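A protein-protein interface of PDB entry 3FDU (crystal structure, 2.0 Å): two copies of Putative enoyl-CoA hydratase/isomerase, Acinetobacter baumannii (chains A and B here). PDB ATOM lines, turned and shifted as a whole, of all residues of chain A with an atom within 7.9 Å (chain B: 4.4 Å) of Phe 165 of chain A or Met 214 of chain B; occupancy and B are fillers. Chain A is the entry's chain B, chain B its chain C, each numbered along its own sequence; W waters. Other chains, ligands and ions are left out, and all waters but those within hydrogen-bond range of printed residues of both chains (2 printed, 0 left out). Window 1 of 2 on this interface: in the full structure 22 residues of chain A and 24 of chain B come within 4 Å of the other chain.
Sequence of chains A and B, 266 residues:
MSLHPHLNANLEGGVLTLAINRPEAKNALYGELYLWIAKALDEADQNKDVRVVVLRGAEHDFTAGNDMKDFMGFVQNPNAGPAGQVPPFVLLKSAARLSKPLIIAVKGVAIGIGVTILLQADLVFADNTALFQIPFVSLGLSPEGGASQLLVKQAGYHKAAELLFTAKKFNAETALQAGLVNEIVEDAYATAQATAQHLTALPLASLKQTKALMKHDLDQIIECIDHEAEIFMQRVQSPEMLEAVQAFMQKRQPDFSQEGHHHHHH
No position is printed for both chains.
Of the 28 pairs that touch across the chains among the printed residues, none has its exchanged pair printed and touching as well.
Water W1 bridges O of Ser 148 of chain A and O of Met 214 of chain B.
Water W2 lies within hydrogen-bond range of the side-chain hydroxyl (OG) of Ser 148 of chain A (2.9 Å), the backbone carbonyl oxygen (O) of Leu 213 of chain B (2.9 Å) and the side-chain amide nitrogen (NE2) of Gln 149 of chain A (2.9 Å).
CG1 of Val 137 of chain A touches CD2 of Leu 207 of chain B (3.9 Å).
Thr 210 of chain B touches Val 137 of chain A (OG1 to CG2, 3.7 Å).
Ser 148 of chain A touches Met 214 of chain B (O to CA, 3.5 Å).
Gln 149 of chain A touches His 216 of chain B.
Lys 215 of chain B touches Tyr 157 of chain A.
Met 214 of chain B touches Ala 160 of chain A.
CB of Ala 161 of chain A touches O of Asp 122 of chain B, at 3.6 Å.
Ala 161 of chain A touches Met 214 of chain B.
Phe 165 of chain A touches Leu 199 of chain B (O to CD2, 3.6 Å).
CB of Lys 211 of chain B touches CZ of Phe 165 of chain A (3.8 Å).
Of the 25 printed residues of chain A, 14 touch a printed residue of chain B.
Printed residues of chain A that touch a printed residue of chain B: Val 137, Ser 138, Pro 143, Ser 148, Gln 149, Val 152, Tyr 157, His 158, Ala 160, Ala 161, Glu 162, Leu 164, Phe 165 and Thr 166.
Printed residues of chain B that touch a printed residue of chain A: Pro 101, Asp 122, Leu 123, Leu 199, Leu 202, Leu 207, Thr 210, Lys 211, Leu 213, Met 214, Lys 215 and His 216.
Hydrophobic or aromatic side chains of chain B within 4 Å of the printed part of chain A: Pro 101, Leu 123, Leu 199, Leu 202, Leu 207, Leu 213, Met 214 and His 216.
Among the printed residues, no Asp or Glu carboxylate lies within 4 Å of a Lys or Arg side-chain nitrogen of the other chain.
The backbone carbonyl oxygen of Pro 135 of chain A sits at hydrogen-bond distance from the side-chain hydroxyl of Ser 138 of chain A, 2.9 Å away.
The side-chain carboxylate (OE2) of Glu 162 of chain A is in salt-bridge range of the side-chain amino group (NZ) of Lys 159 of chain A, 2.9 Å away.
O of Glu 162 of chain A lies within hydrogen-bond range of OG1 of Thr 166 of chain A, 2.8 Å away.
The side-chain amino group (NZ) of Lys 168 of chain A is in salt-bridge range of the side-chain carboxylate (OE1) of Glu 162 of chain A, 2.9 Å away.
The side-chain carboxylate of Asp 122 of chain B is in salt-bridge range of the side-chain amino group of Lys 211 of chain B (2.6 Å).
The side-chain hydroxyl (OH) of Tyr 157 of chain A is in hydrogen-bond range of the side-chain carboxylate (OD1) of Asp 122 of chain B.
Of the printed residues of chain A, Met 214 of chain B touches Ser 148, Val 152, Tyr 157, Ala 160, Ala 161, Leu 164 and Phe 165.
Printed residues of chain A within 4 Å of Asp 122 of chain B: Tyr 157 (2.8 Å), His 158 (3.4 Å), Ala 161 (3.6 Å) and Phe 165 (3.6 Å).
Of the printed residues of chain A, Lys 211 of chain B touches Tyr 157 and Phe 165.
Printed residues of chain B within 4 Å of Tyr 157 of chain A: Asp 122 (2.8 Å), Lys 211 (3.9 Å), Met 214 (3.8 Å) and Lys 215 (3.4 Å).
Printed residues of chain B within 4 Å of Ser 138 of chain A: Leu 202 (3.7 Å).
The nearest printed residue of chain A that does not touch His 216 of chain B is Ser 148 of chain A (5.1 Å).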
ATOM      1  N   ILE A 134     -32.628  -7.387  -0.351  1.00  0.00           N
ATOM      2  CA  ILE A 134     -31.656  -8.009  -1.231  1.00  0.00           C
ATOM      3  C   ILE A 134     -30.296  -7.397  -0.890  1.00  0.00           C
ATOM      4  O   ILE A 134     -29.926  -6.361  -1.429  1.00  0.00           O
ATOM      5  CB  ILE A 134     -31.963  -7.742  -2.755  1.00  0.00           C
ATOM      6  CG1 ILE A 134     -33.475  -7.863  -3.039  1.00  0.00           C
ATOM      7  CG2 ILE A 134     -31.150  -8.669  -3.642  1.00  0.00           C
ATOM      8  CD1 ILE A 134     -33.856  -7.449  -4.454  1.00  0.00           C
ATOM      9  N   PRO A 135     -29.546  -8.034   0.023  1.00  0.00           N
ATOM     10  CA  PRO A 135     -28.375  -7.404   0.606  1.00  0.00           C
ATOM     11  C   PRO A 135     -27.140  -7.600  -0.245  1.00  0.00           C
ATOM     12  O   PRO A 135     -26.079  -7.076   0.113  1.00  0.00           O
ATOM     13  CB  PRO A 135     -28.197  -8.146   1.959  1.00  0.00           C
ATOM     14  CG  PRO A 135     -28.705  -9.539   1.690  1.00  0.00           C
ATOM     15  CD  PRO A 135     -29.753  -9.407   0.531  1.00  0.00           C
ATOM     16  N   PHE A 136     -27.263  -8.334  -1.356  1.00  0.00           N
ATOM     17  CA  PHE A 136     -26.075  -8.740  -2.117  1.00  0.00           C
ATOM     18  C   PHE A 136     -25.077  -7.628  -2.415  1.00  0.00           C
ATOM     19  O   PHE A 136     -23.873  -7.869  -2.298  1.00  0.00           O
ATOM     20  CB  PHE A 136     -26.417  -9.431  -3.434  1.00  0.00           C
ATOM     21  CG  PHE A 136     -27.353 -10.556  -3.290  1.00  0.00           C
ATOM     22  CD1 PHE A 136     -27.153 -11.521  -2.330  1.00  0.00           C
ATOM     23  CD2 PHE A 136     -28.448 -10.653  -4.127  1.00  0.00           C
ATOM     24  CE1 PHE A 136     -28.047 -12.578  -2.198  1.00  0.00           C
ATOM     25  CE2 PHE A 136     -29.338 -11.701  -4.005  1.00  0.00           C
ATOM     26  CZ  PHE A 136     -29.146 -12.652  -3.050  1.00  0.00           C
ATOM     27  N   VAL A 137     -25.541  -6.449  -2.857  1.00  0.00           N
ATOM     28  CA  VAL A 137     -24.601  -5.371  -3.177  1.00  0.00           C
ATOM     29  C   VAL A 137     -23.788  -4.936  -1.977  1.00  0.00           C
ATOM     30  O   VAL A 137     -22.569  -4.679  -2.105  1.00  0.00           O
ATOM     31  CB  VAL A 137     -25.244  -4.113  -3.796  1.00  0.00           C
ATOM     32  CG1 VAL A 137     -24.279  -2.885  -3.598  1.00  0.00           C
ATOM     33  CG2 VAL A 137     -25.503  -4.327  -5.266  1.00  0.00           C
ATOM     34  N   SER A 138     -24.444  -4.833  -0.822  1.00  0.00           N
ATOM     35  CA  SER A 138     -23.730  -4.444   0.381  1.00  0.00           C
ATOM     36  C   SER A 138     -22.872  -5.559   1.020  1.00  0.00           C
ATOM     37  O   SER A 138     -22.186  -5.315   2.022  1.00  0.00           O
ATOM     38  CB  SER A 138     -24.670  -3.846   1.419  1.00  0.00           C
ATOM     39  OG  SER A 138     -25.685  -4.770   1.760  1.00  0.00           O
ATOM     40  N   PRO A 143     -26.000 -10.084  -8.113  1.00  0.00           N
ATOM     41  CA  PRO A 143     -27.366 -10.652  -8.074  1.00  0.00           C
ATOM     42  C   PRO A 143     -27.408 -12.179  -8.192  1.00  0.00           C
ATOM     43  O   PRO A 143     -26.477 -12.792  -8.714  1.00  0.00           O
ATOM     44  CB  PRO A 143     -28.037 -10.017  -9.301  1.00  0.00           C
ATOM     45  CG  PRO A 143     -27.266  -8.671  -9.464  1.00  0.00           C
ATOM     46  CD  PRO A 143     -25.834  -9.143  -9.229  1.00  0.00           C
ATOM     47  N   ALA A 147     -32.333 -12.430 -10.959  1.00  0.00           N
ATOM     48  CA  ALA A 147     -32.908 -11.139 -10.564  1.00  0.00           C
ATOM     49  C   ALA A 147     -32.539  -9.975 -11.495  1.00  0.00           C
ATOM     50  O   ALA A 147     -33.307  -9.025 -11.630  1.00  0.00           O
ATOM     51  CB  ALA A 147     -32.510 -10.792  -9.134  1.00  0.00           C
ATOM     52  N   SER A 148     -31.369 -10.030 -12.133  1.00  0.00           N
ATOM     53  CA  SER A 148     -30.931  -8.888 -12.935  1.00  0.00           C
ATOM     54  C   SER A 148     -31.766  -8.738 -14.239  1.00  0.00           C
ATOM     55  O   SER A 148     -31.700  -7.710 -14.931  1.00  0.00           O
ATOM     56  CB  SER A 148     -29.453  -9.022 -13.252  1.00  0.00           C
ATOM     57  OG  SER A 148     -29.259 -10.052 -14.218  1.00  0.00           O
ATOM     58  N   GLN A 149     -32.527  -9.774 -14.580  1.00  0.00           N
ATOM     59  CA  GLN A 149     -33.477  -9.721 -15.716  1.00  0.00           C
ATOM     60  C   GLN A 149     -34.910  -9.837 -15.194  1.00  0.00           C
ATOM     61  O   GLN A 149     -35.778  -9.027 -15.562  1.00  0.00           O
ATOM     62  CB  GLN A 149     -33.162 -10.784 -16.775  1.00  0.00           C
ATOM     63  CG  GLN A 149     -31.736 -10.654 -17.390  1.00  0.00           C
ATOM     64  CD  GLN A 149     -31.495 -11.580 -18.612  1.00  0.00           C
ATOM     65  OE1 GLN A 149     -32.423 -12.212 -19.132  1.00  0.00           O
ATOM     66  NE2 GLN A 149     -30.228 -11.644 -19.065  1.00  0.00           N
ATOM     67  N   LEU A 151     -36.193  -9.225 -12.100  1.00  0.00           N
ATOM     68  CA  LEU A 151     -36.690  -8.156 -11.273  1.00  0.00           C
ATOM     69  C   LEU A 151     -36.932  -6.879 -12.132  1.00  0.00           C
ATOM     70  O   LEU A 151     -37.893  -6.122 -11.905  1.00  0.00           O
ATOM     71  CB  LEU A 151     -35.724  -7.898 -10.092  1.00  0.00           C
ATOM     72  CG  LEU A 151     -36.254  -6.849  -9.101  1.00  0.00           C
ATOM     73  CD1 LEU A 151     -37.498  -7.307  -8.336  1.00  0.00           C
ATOM     74  CD2 LEU A 151     -35.143  -6.359  -8.085  1.00  0.00           C
ATOM     75  N   VAL A 152     -36.079  -6.662 -13.136  1.00  0.00           N
ATOM     76  CA  VAL A 152     -36.275  -5.543 -14.085  1.00  0.00           C
ATOM     77  C   VAL A 152     -37.592  -5.706 -14.800  1.00  0.00           C
ATOM     78  O   VAL A 152     -38.361  -4.744 -14.924  1.00  0.00           O
ATOM     79  CB  VAL A 152     -35.162  -5.444 -15.127  1.00  0.00           C
ATOM     80  CG1 VAL A 152     -35.599  -4.468 -16.278  1.00  0.00           C
ATOM     81  CG2 VAL A 152     -33.855  -4.954 -14.435  1.00  0.00           C
ATOM     82  N   GLY A 156     -40.005  -3.202 -13.222  1.00  0.00           N
ATOM     83  CA  GLY A 156     -39.575  -2.088 -14.071  1.00  0.00           C
ATOM     84  C   GLY A 156     -38.128  -1.759 -13.707  1.00  0.00           C
ATOM     85  O   GLY A 156     -37.682  -2.000 -12.586  1.00  0.00           O
ATOM     86  N   TYR A 157     -37.392  -1.184 -14.646  1.00  0.00           N
ATOM     87  CA  TYR A 157     -35.953  -0.970 -14.421  1.00  0.00           C
ATOM     88  C   TYR A 157     -35.633  -0.049 -13.241  1.00  0.00           C
ATOM     89  O   TYR A 157     -34.799  -0.380 -12.422  1.00  0.00           O
ATOM     90  CB  TYR A 157     -35.274  -0.418 -15.685  1.00  0.00           C
ATOM     91  CG  TYR A 157     -33.753  -0.328 -15.515  1.00  0.00           C
ATOM     92  CD1 TYR A 157     -32.925  -1.324 -15.996  1.00  0.00           C
ATOM     93  CD2 TYR A 157     -33.165   0.758 -14.861  1.00  0.00           C
ATOM     94  CE1 TYR A 157     -31.513  -1.238 -15.845  1.00  0.00           C
ATOM     95  CE2 TYR A 157     -31.765   0.837 -14.667  1.00  0.00           C
ATOM     96  CZ  TYR A 157     -30.953  -0.167 -15.172  1.00  0.00           C
ATOM     97  OH  TYR A 157     -29.585  -0.081 -14.999  1.00  0.00           O
ATOM     98  N   HIS A 158     -36.291   1.105 -13.172  1.00  0.00           N
ATOM     99  CA  HIS A 158     -36.005   2.069 -12.100  1.00  0.00           C
ATOM    100  C   HIS A 158     -36.177   1.468 -10.677  1.00  0.00           C
ATOM    101  O   HIS A 158     -35.290   1.630  -9.795  1.00  0.00           O
ATOM    102  CB  HIS A 158     -36.837   3.361 -12.257  1.00  0.00           C
ATOM    103  CG  HIS A 158     -36.342   4.281 -13.327  1.00  0.00           C
ATOM    104  ND1 HIS A 158     -37.157   5.197 -13.961  1.00  0.00           N
ATOM    105  CD2 HIS A 158     -35.111   4.421 -13.885  1.00  0.00           C
ATOM    106  CE1 HIS A 158     -36.448   5.870 -14.853  1.00  0.00           C
ATOM    107  NE2 HIS A 158     -35.204   5.415 -14.826  1.00  0.00           N
ATOM    108  N   LYS A 159     -37.294   0.794 -10.441  1.00  0.00           N
ATOM    109  CA  LYS A 159     -37.515   0.214  -9.113  1.00  0.00           C
ATOM    110  C   LYS A 159     -36.547  -0.955  -8.786  1.00  0.00           C
ATOM    111  O   LYS A 159     -36.132  -1.102  -7.632  1.00  0.00           O
ATOM    112  CB  LYS A 159     -38.965  -0.220  -8.936  1.00  0.00           C
ATOM    113  CG  LYS A 159     -39.360  -0.623  -7.506  1.00  0.00           C
ATOM    114  CD  LYS A 159     -39.262   0.530  -6.502  1.00  0.00           C
ATOM    115  CE  LYS A 159     -40.132   1.732  -6.940  1.00  0.00           C
ATOM    116  NZ  LYS A 159     -39.945   2.910  -5.966  1.00  0.00           N
ATOM    117  N   ALA A 160     -36.223  -1.765  -9.790  1.00  0.00           N
ATOM    118  CA  ALA A 160     -35.309  -2.915  -9.650  1.00  0.00           C
ATOM    119  C   ALA A 160     -33.943  -2.375  -9.263  1.00  0.00           C
ATOM    120  O   ALA A 160     -33.248  -2.923  -8.388  1.00  0.00           O
ATOM    121  CB  ALA A 160     -35.182  -3.665 -10.982  1.00  0.00           C
ATOM    122  N   ALA A 161     -33.553  -1.291  -9.930  1.00  0.00           N
ATOM    123  CA  ALA A 161     -32.274  -0.651  -9.611  1.00  0.00           C
ATOM    124  C   ALA A 161     -32.281  -0.104  -8.202  1.00  0.00           C
ATOM    125  O   ALA A 161     -31.318  -0.253  -7.454  1.00  0.00           O
ATOM    126  CB  ALA A 161     -31.900   0.416 -10.660  1.00  0.00           C
ATOM    127  N   GLU A 162     -33.381   0.482  -7.790  1.00  0.00           N
ATOM    128  CA  GLU A 162     -33.478   0.959  -6.429  1.00  0.00           C
ATOM    129  C   GLU A 162     -33.260  -0.196  -5.411  1.00  0.00           C
ATOM    130  O   GLU A 162     -32.431  -0.101  -4.514  1.00  0.00           O
ATOM    131  CB  GLU A 162     -34.848   1.616  -6.231  1.00  0.00           C
ATOM    132  CG  GLU A 162     -35.076   2.233  -4.852  1.00  0.00           C
ATOM    133  CD  GLU A 162     -36.460   2.845  -4.720  1.00  0.00           C
ATOM    134  OE1 GLU A 162     -36.937   2.983  -3.578  1.00  0.00           O
ATOM    135  OE2 GLU A 162     -37.085   3.164  -5.765  1.00  0.00           O
ATOM    136  N   LEU A 163     -33.984  -1.287  -5.572  1.00  0.00           N
ATOM    137  CA  LEU A 163     -33.851  -2.438  -4.673  1.00  0.00           C
ATOM    138  C   LEU A 163     -32.477  -3.140  -4.741  1.00  0.00           C
ATOM    139  O   LEU A 163     -31.903  -3.467  -3.691  1.00  0.00           O
ATOM    140  CB  LEU A 163     -34.999  -3.439  -4.900  1.00  0.00           C
ATOM    141  CG  LEU A 163     -36.434  -2.846  -4.814  1.00  0.00           C
ATOM    142  CD1 LEU A 163     -37.523  -3.945  -4.980  1.00  0.00           C
ATOM    143  CD2 LEU A 163     -36.720  -2.006  -3.528  1.00  0.00           C
ATOM    144  N   LEU A 164     -31.955  -3.373  -5.945  1.00  0.00           N
ATOM    145  CA  LEU A 164     -30.636  -3.972  -6.103  1.00  0.00           C
ATOM    146  C   LEU A 164     -29.489  -3.066  -5.652  1.00  0.00           C
ATOM    147  O   LEU A 164     -28.671  -3.476  -4.811  1.00  0.00           O
ATOM    148  CB  LEU A 164     -30.419  -4.458  -7.540  1.00  0.00           C
ATOM    149  CG  LEU A 164     -31.319  -5.647  -7.833  1.00  0.00           C
ATOM    150  CD1 LEU A 164     -31.349  -6.073  -9.310  1.00  0.00           C
ATOM    151  CD2 LEU A 164     -30.854  -6.817  -6.898  1.00  0.00           C
ATOM    152  N   PHE A 165     -29.400  -1.856  -6.208  1.00  0.00           N
ATOM    153  CA  PHE A 165     -28.285  -0.940  -5.885  1.00  0.00           C
ATOM    154  C   PHE A 165     -28.193  -0.597  -4.403  1.00  0.00           C
ATOM    155  O   PHE A 165     -27.080  -0.610  -3.833  1.00  0.00           O
ATOM    156  CB  PHE A 165     -28.421   0.402  -6.623  1.00  0.00           C
ATOM    157  CG  PHE A 165     -28.111   0.349  -8.069  1.00  0.00           C
ATOM    158  CD1 PHE A 165     -28.038  -0.856  -8.746  1.00  0.00           C
ATOM    159  CD2 PHE A 165     -27.935   1.526  -8.781  1.00  0.00           C
ATOM    160  CE1 PHE A 165     -27.764  -0.896 -10.097  1.00  0.00           C
ATOM    161  CE2 PHE A 165     -27.665   1.520 -10.127  1.00  0.00           C
ATOM    162  CZ  PHE A 165     -27.581   0.298 -10.812  1.00  0.00           C
ATOM    163  N   THR A 166     -29.334  -0.260  -3.783  1.00  0.00           N
ATOM    164  CA  THR A 166     -29.335   0.277  -2.420  1.00  0.00           C
ATOM    165  C   THR A 166     -29.244  -0.822  -1.346  1.00  0.00           C
ATOM    166  O   THR A 166     -28.829  -0.540  -0.235  1.00  0.00           O
ATOM    167  CB  THR A 166     -30.569   1.220  -2.066  1.00  0.00           C
ATOM    168  OG1 THR A 166     -31.785   0.458  -1.886  1.00  0.00           O
ATOM    169  CG2 THR A 166     -30.812   2.346  -3.113  1.00  0.00           C
ATOM    170  N   ALA A 167     -29.669  -2.040  -1.682  1.00  0.00           N
ATOM    171  CA  ALA A 167     -29.672  -3.149  -0.733  1.00  0.00           C
ATOM    172  C   ALA A 167     -30.525  -2.881   0.494  1.00  0.00           C
ATOM    173  O   ALA A 167     -30.364  -3.527   1.533  1.00  0.00           O
ATOM    174  CB  ALA A 167     -28.225  -3.533  -0.321  1.00  0.00           C
ATOM    175  N   LYS A 168     -31.433  -1.930   0.392  1.00  0.00           N
ATOM    176  CA  LYS A 168     -32.247  -1.560   1.552  1.00  0.00           C
ATOM    177  C   LYS A 168     -33.328  -2.597   1.942  1.00  0.00           C
ATOM    178  O   LYS A 168     -33.800  -3.377   1.114  1.00  0.00           O
ATOM    179  CB  LYS A 168     -32.911  -0.203   1.296  1.00  0.00           C
ATOM    180  CG  LYS A 168     -34.155  -0.248   0.390  1.00  0.00           C
ATOM    181  CD  LYS A 168     -34.298   1.078  -0.344  1.00  0.00           C
ATOM    182  CE  LYS A 168     -35.696   1.351  -0.766  1.00  0.00           C
ATOM    183  NZ  LYS A 168     -35.777   2.839  -0.956  1.00  0.00           N
ATOM    184  N   GLU A 228     -25.264 -15.568 -13.831  1.00  0.00           N
ATOM    185  CA  GLU A 228     -25.142 -14.857 -12.571  1.00  0.00           C
ATOM    186  C   GLU A 228     -24.329 -15.652 -11.550  1.00  0.00           C
ATOM    187  O   GLU A 228     -23.547 -15.077 -10.795  1.00  0.00           O
ATOM    188  CB  GLU A 228     -26.509 -14.572 -11.971  1.00  0.00           C
ATOM    189  CG  GLU A 228     -27.207 -13.337 -12.588  1.00  0.00           C
ATOM    190  CD  GLU A 228     -28.575 -13.135 -11.992  1.00  0.00           C
ATOM    191  OE1 GLU A 228     -28.985 -14.028 -11.214  1.00  0.00           O
ATOM    192  OE2 GLU A 228     -29.232 -12.102 -12.313  1.00  0.00           O
ATOM    193  N   PRO B 101     -23.583   4.360 -11.320  1.00  0.00           N
ATOM    194  CA  PRO B 101     -24.991   4.743 -11.176  1.00  0.00           C
ATOM    195  C   PRO B 101     -25.227   6.186 -11.594  1.00  0.00           C
ATOM    196  O   PRO B 101     -24.422   7.083 -11.275  1.00  0.00           O
ATOM    197  CB  PRO B 101     -25.258   4.586  -9.676  1.00  0.00           C
ATOM    198  CG  PRO B 101     -24.129   3.593  -9.187  1.00  0.00           C
ATOM    199  CD  PRO B 101     -22.950   3.987 -10.037  1.00  0.00           C
ATOM    200  N   ASP B 122     -30.638   5.321 -13.690  1.00  0.00           N
ATOM    201  CA  ASP B 122     -30.961   4.210 -12.808  1.00  0.00           C
ATOM    202  C   ASP B 122     -31.993   4.561 -11.774  1.00  0.00           C
ATOM    203  O   ASP B 122     -32.858   3.743 -11.487  1.00  0.00           O
ATOM    204  CB  ASP B 122     -29.697   3.672 -12.134  1.00  0.00           C
ATOM    205  CG  ASP B 122     -28.610   3.337 -13.155  1.00  0.00           C
ATOM    206  OD1 ASP B 122     -28.844   2.460 -14.036  1.00  0.00           O
ATOM    207  OD2 ASP B 122     -27.535   3.984 -13.119  1.00  0.00           O
ATOM    208  N   LEU B 123     -31.921   5.786 -11.247  1.00  0.00           N
ATOM    209  CA  LEU B 123     -32.860   6.296 -10.241  1.00  0.00           C
ATOM    210  C   LEU B 123     -33.328   7.746 -10.544  1.00  0.00           C
ATOM    211  O   LEU B 123     -32.531   8.587 -10.960  1.00  0.00           O
ATOM    212  CB  LEU B 123     -32.227   6.226  -8.858  1.00  0.00           C
ATOM    213  CG  LEU B 123     -31.660   4.837  -8.491  1.00  0.00           C
ATOM    214  CD1 LEU B 123     -30.428   4.889  -7.573  1.00  0.00           C
ATOM    215  CD2 LEU B 123     -32.793   4.075  -7.823  1.00  0.00           C
ATOM    216  N   LEU B 199     -24.873   5.152  -1.956  1.00  0.00           N
ATOM    217  CA  LEU B 199     -24.247   4.350  -3.000  1.00  0.00           C
ATOM    218  C   LEU B 199     -22.704   4.481  -3.079  1.00  0.00           C
ATOM    219  O   LEU B 199     -22.035   3.489  -3.368  1.00  0.00           O
ATOM    220  CB  LEU B 199     -24.870   4.582  -4.374  1.00  0.00           C
ATOM    221  CG  LEU B 199     -26.390   4.369  -4.612  1.00  0.00           C
ATOM    222  CD1 LEU B 199     -26.708   4.631  -6.119  1.00  0.00           C
ATOM    223  CD2 LEU B 199     -26.833   2.980  -4.157  1.00  0.00           C
ATOM    224  N   LEU B 202     -20.897   2.030  -0.870  1.00  0.00           N
ATOM    225  CA  LEU B 202     -21.019   0.622  -1.181  1.00  0.00           C
ATOM    226  C   LEU B 202     -19.976   0.214  -2.234  1.00  0.00           C
ATOM    227  O   LEU B 202     -19.394   1.061  -2.934  1.00  0.00           O
ATOM    228  CB  LEU B 202     -22.475   0.250  -1.616  1.00  0.00           C
ATOM    229  CG  LEU B 202     -23.672   0.433  -0.644  1.00  0.00           C
ATOM    230  CD1 LEU B 202     -25.091   0.257  -1.336  1.00  0.00           C
ATOM    231  CD2 LEU B 202     -23.622  -0.438   0.622  1.00  0.00           C
ATOM    232  N   LEU B 207     -21.694  -2.604  -7.607  1.00  0.00           N
ATOM    233  CA  LEU B 207     -22.623  -1.744  -8.348  1.00  0.00           C
ATOM    234  C   LEU B 207     -22.369  -1.845  -9.833  1.00  0.00           C
ATOM    235  O   LEU B 207     -23.303  -2.026 -10.624  1.00  0.00           O
ATOM    236  CB  LEU B 207     -22.509  -0.300  -7.887  1.00  0.00           C
ATOM    237  CG  LEU B 207     -23.061  -0.131  -6.498  1.00  0.00           C
ATOM    238  CD1 LEU B 207     -22.607   1.226  -5.937  1.00  0.00           C
ATOM    239  CD2 LEU B 207     -24.593  -0.275  -6.511  1.00  0.00           C
ATOM    240  N   THR B 210     -23.468  -5.369 -11.073  1.00  0.00           N
ATOM    241  CA  THR B 210     -24.936  -5.482 -11.020  1.00  0.00           C
ATOM    242  C   THR B 210     -25.588  -4.708 -12.175  1.00  0.00           C
ATOM    243  O   THR B 210     -26.459  -5.216 -12.850  1.00  0.00           O
ATOM    244  CB  THR B 210     -25.472  -4.971  -9.707  1.00  0.00           C
ATOM    245  OG1 THR B 210     -25.008  -5.817  -8.649  1.00  0.00           O
ATOM    246  CG2 THR B 210     -26.971  -4.983  -9.696  1.00  0.00           C
ATOM    247  N   LYS B 211     -25.126  -3.489 -12.419  1.00  0.00           N
ATOM    248  CA  LYS B 211     -25.684  -2.661 -13.504  1.00  0.00           C
ATOM    249  C   LYS B 211     -25.390  -3.248 -14.865  1.00  0.00           C
ATOM    250  O   LYS B 211     -26.237  -3.233 -15.770  1.00  0.00           O
ATOM    251  CB  LYS B 211     -25.189  -1.203 -13.402  1.00  0.00           C
ATOM    252  CG  LYS B 211     -25.686  -0.317 -14.545  1.00  0.00           C
ATOM    253  CD  LYS B 211     -25.543   1.189 -14.260  1.00  0.00           C
ATOM    254  CE  LYS B 211     -26.048   2.048 -15.431  1.00  0.00           C
ATOM    255  NZ  LYS B 211     -25.854   3.520 -15.089  1.00  0.00           N
ATOM    256  N   ALA B 212     -24.179  -3.770 -15.036  1.00  0.00           N
ATOM    257  CA  ALA B 212     -23.816  -4.361 -16.329  1.00  0.00           C
ATOM    258  C   ALA B 212     -24.723  -5.581 -16.641  1.00  0.00           C
ATOM    259  O   ALA B 212     -25.121  -5.786 -17.790  1.00  0.00           O
ATOM    260  CB  ALA B 212     -22.299  -4.728 -16.372  1.00  0.00           C
ATOM    261  N   LEU B 213     -25.063  -6.368 -15.621  1.00  0.00           N
ATOM    262  CA  LEU B 213     -26.009  -7.480 -15.824  1.00  0.00           C
ATOM    263  C   LEU B 213     -27.415  -6.963 -16.161  1.00  0.00           C
ATOM    264  O   LEU B 213     -28.049  -7.469 -17.073  1.00  0.00           O
ATOM    265  CB  LEU B 213     -26.070  -8.386 -14.580  1.00  0.00           C
ATOM    266  CG  LEU B 213     -24.862  -9.316 -14.362  1.00  0.00           C
ATOM    267  CD1 LEU B 213     -24.799  -9.831 -12.899  1.00  0.00           C
ATOM    268  CD2 LEU B 213     -24.965 -10.466 -15.348  1.00  0.00           C
ATOM    269  N   MET B 214     -27.893  -5.975 -15.390  1.00  0.00           N
ATOM    270  CA  MET B 214     -29.185  -5.328 -15.676  1.00  0.00           C
ATOM    271  C   MET B 214     -29.257  -4.743 -17.080  1.00  0.00           C
ATOM    272  O   MET B 214     -30.309  -4.827 -17.745  1.00  0.00           O
ATOM    273  CB  MET B 214     -29.466  -4.244 -14.632  1.00  0.00           C
ATOM    274  CG  MET B 214     -29.680  -4.784 -13.216  1.00  0.00           C
ATOM    275  SD  MET B 214     -29.933  -3.506 -11.958  1.00  0.00           S
ATOM    276  CE  MET B 214     -31.608  -3.040 -12.324  1.00  0.00           C
ATOM    277  N   LYS B 215     -28.149  -4.168 -17.553  1.00  0.00           N
ATOM    278  CA  LYS B 215     -28.074  -3.682 -18.937  1.00  0.00           C
ATOM    279  C   LYS B 215     -27.257  -4.553 -19.899  1.00  0.00           C
ATOM    280  O   LYS B 215     -26.494  -4.051 -20.738  1.00  0.00           O
ATOM    281  CB  LYS B 215     -27.611  -2.228 -18.959  1.00  0.00           C
ATOM    282  CG  LYS B 215     -28.318  -1.384 -17.885  1.00  0.00           C
ATOM    283  CD  LYS B 215     -27.966   0.086 -18.050  1.00  0.00           C
ATOM    284  CE  LYS B 215     -28.539   0.637 -19.361  1.00  0.00           C
ATOM    285  NZ  LYS B 215     -28.431   2.158 -19.374  1.00  0.00           N
ATOM    286  N   HIS B 216     -27.475  -5.858 -19.801  1.00  0.00           N
ATOM    287  CA  HIS B 216     -26.857  -6.834 -20.692  1.00  0.00           C
ATOM    288  C   HIS B 216     -27.155  -6.541 -22.152  1.00  0.00           C
ATOM    289  O   HIS B 216     -26.375  -6.899 -23.044  1.00  0.00           O
ATOM    290  CB  HIS B 216     -27.354  -8.256 -20.358  1.00  0.00           C
ATOM    291  CG  HIS B 216     -28.839  -8.428 -20.492  1.00  0.00           C
ATOM    292  ND1 HIS B 216     -29.431  -8.897 -21.642  1.00  0.00           N
ATOM    293  CD2 HIS B 216     -29.855  -8.147 -19.639  1.00  0.00           C
ATOM    294  CE1 HIS B 216     -30.745  -8.919 -21.491  1.00  0.00           C
ATOM    295  NE2 HIS B 216     -31.029  -8.459 -20.290  1.00  0.00           N
HETATM  296  O   HOH W   1     -32.275  -6.713 -17.259  1.00  0.00           O
HETATM  297  O   HOH W   2     -28.590 -10.328 -17.000  1.00  0.00           O
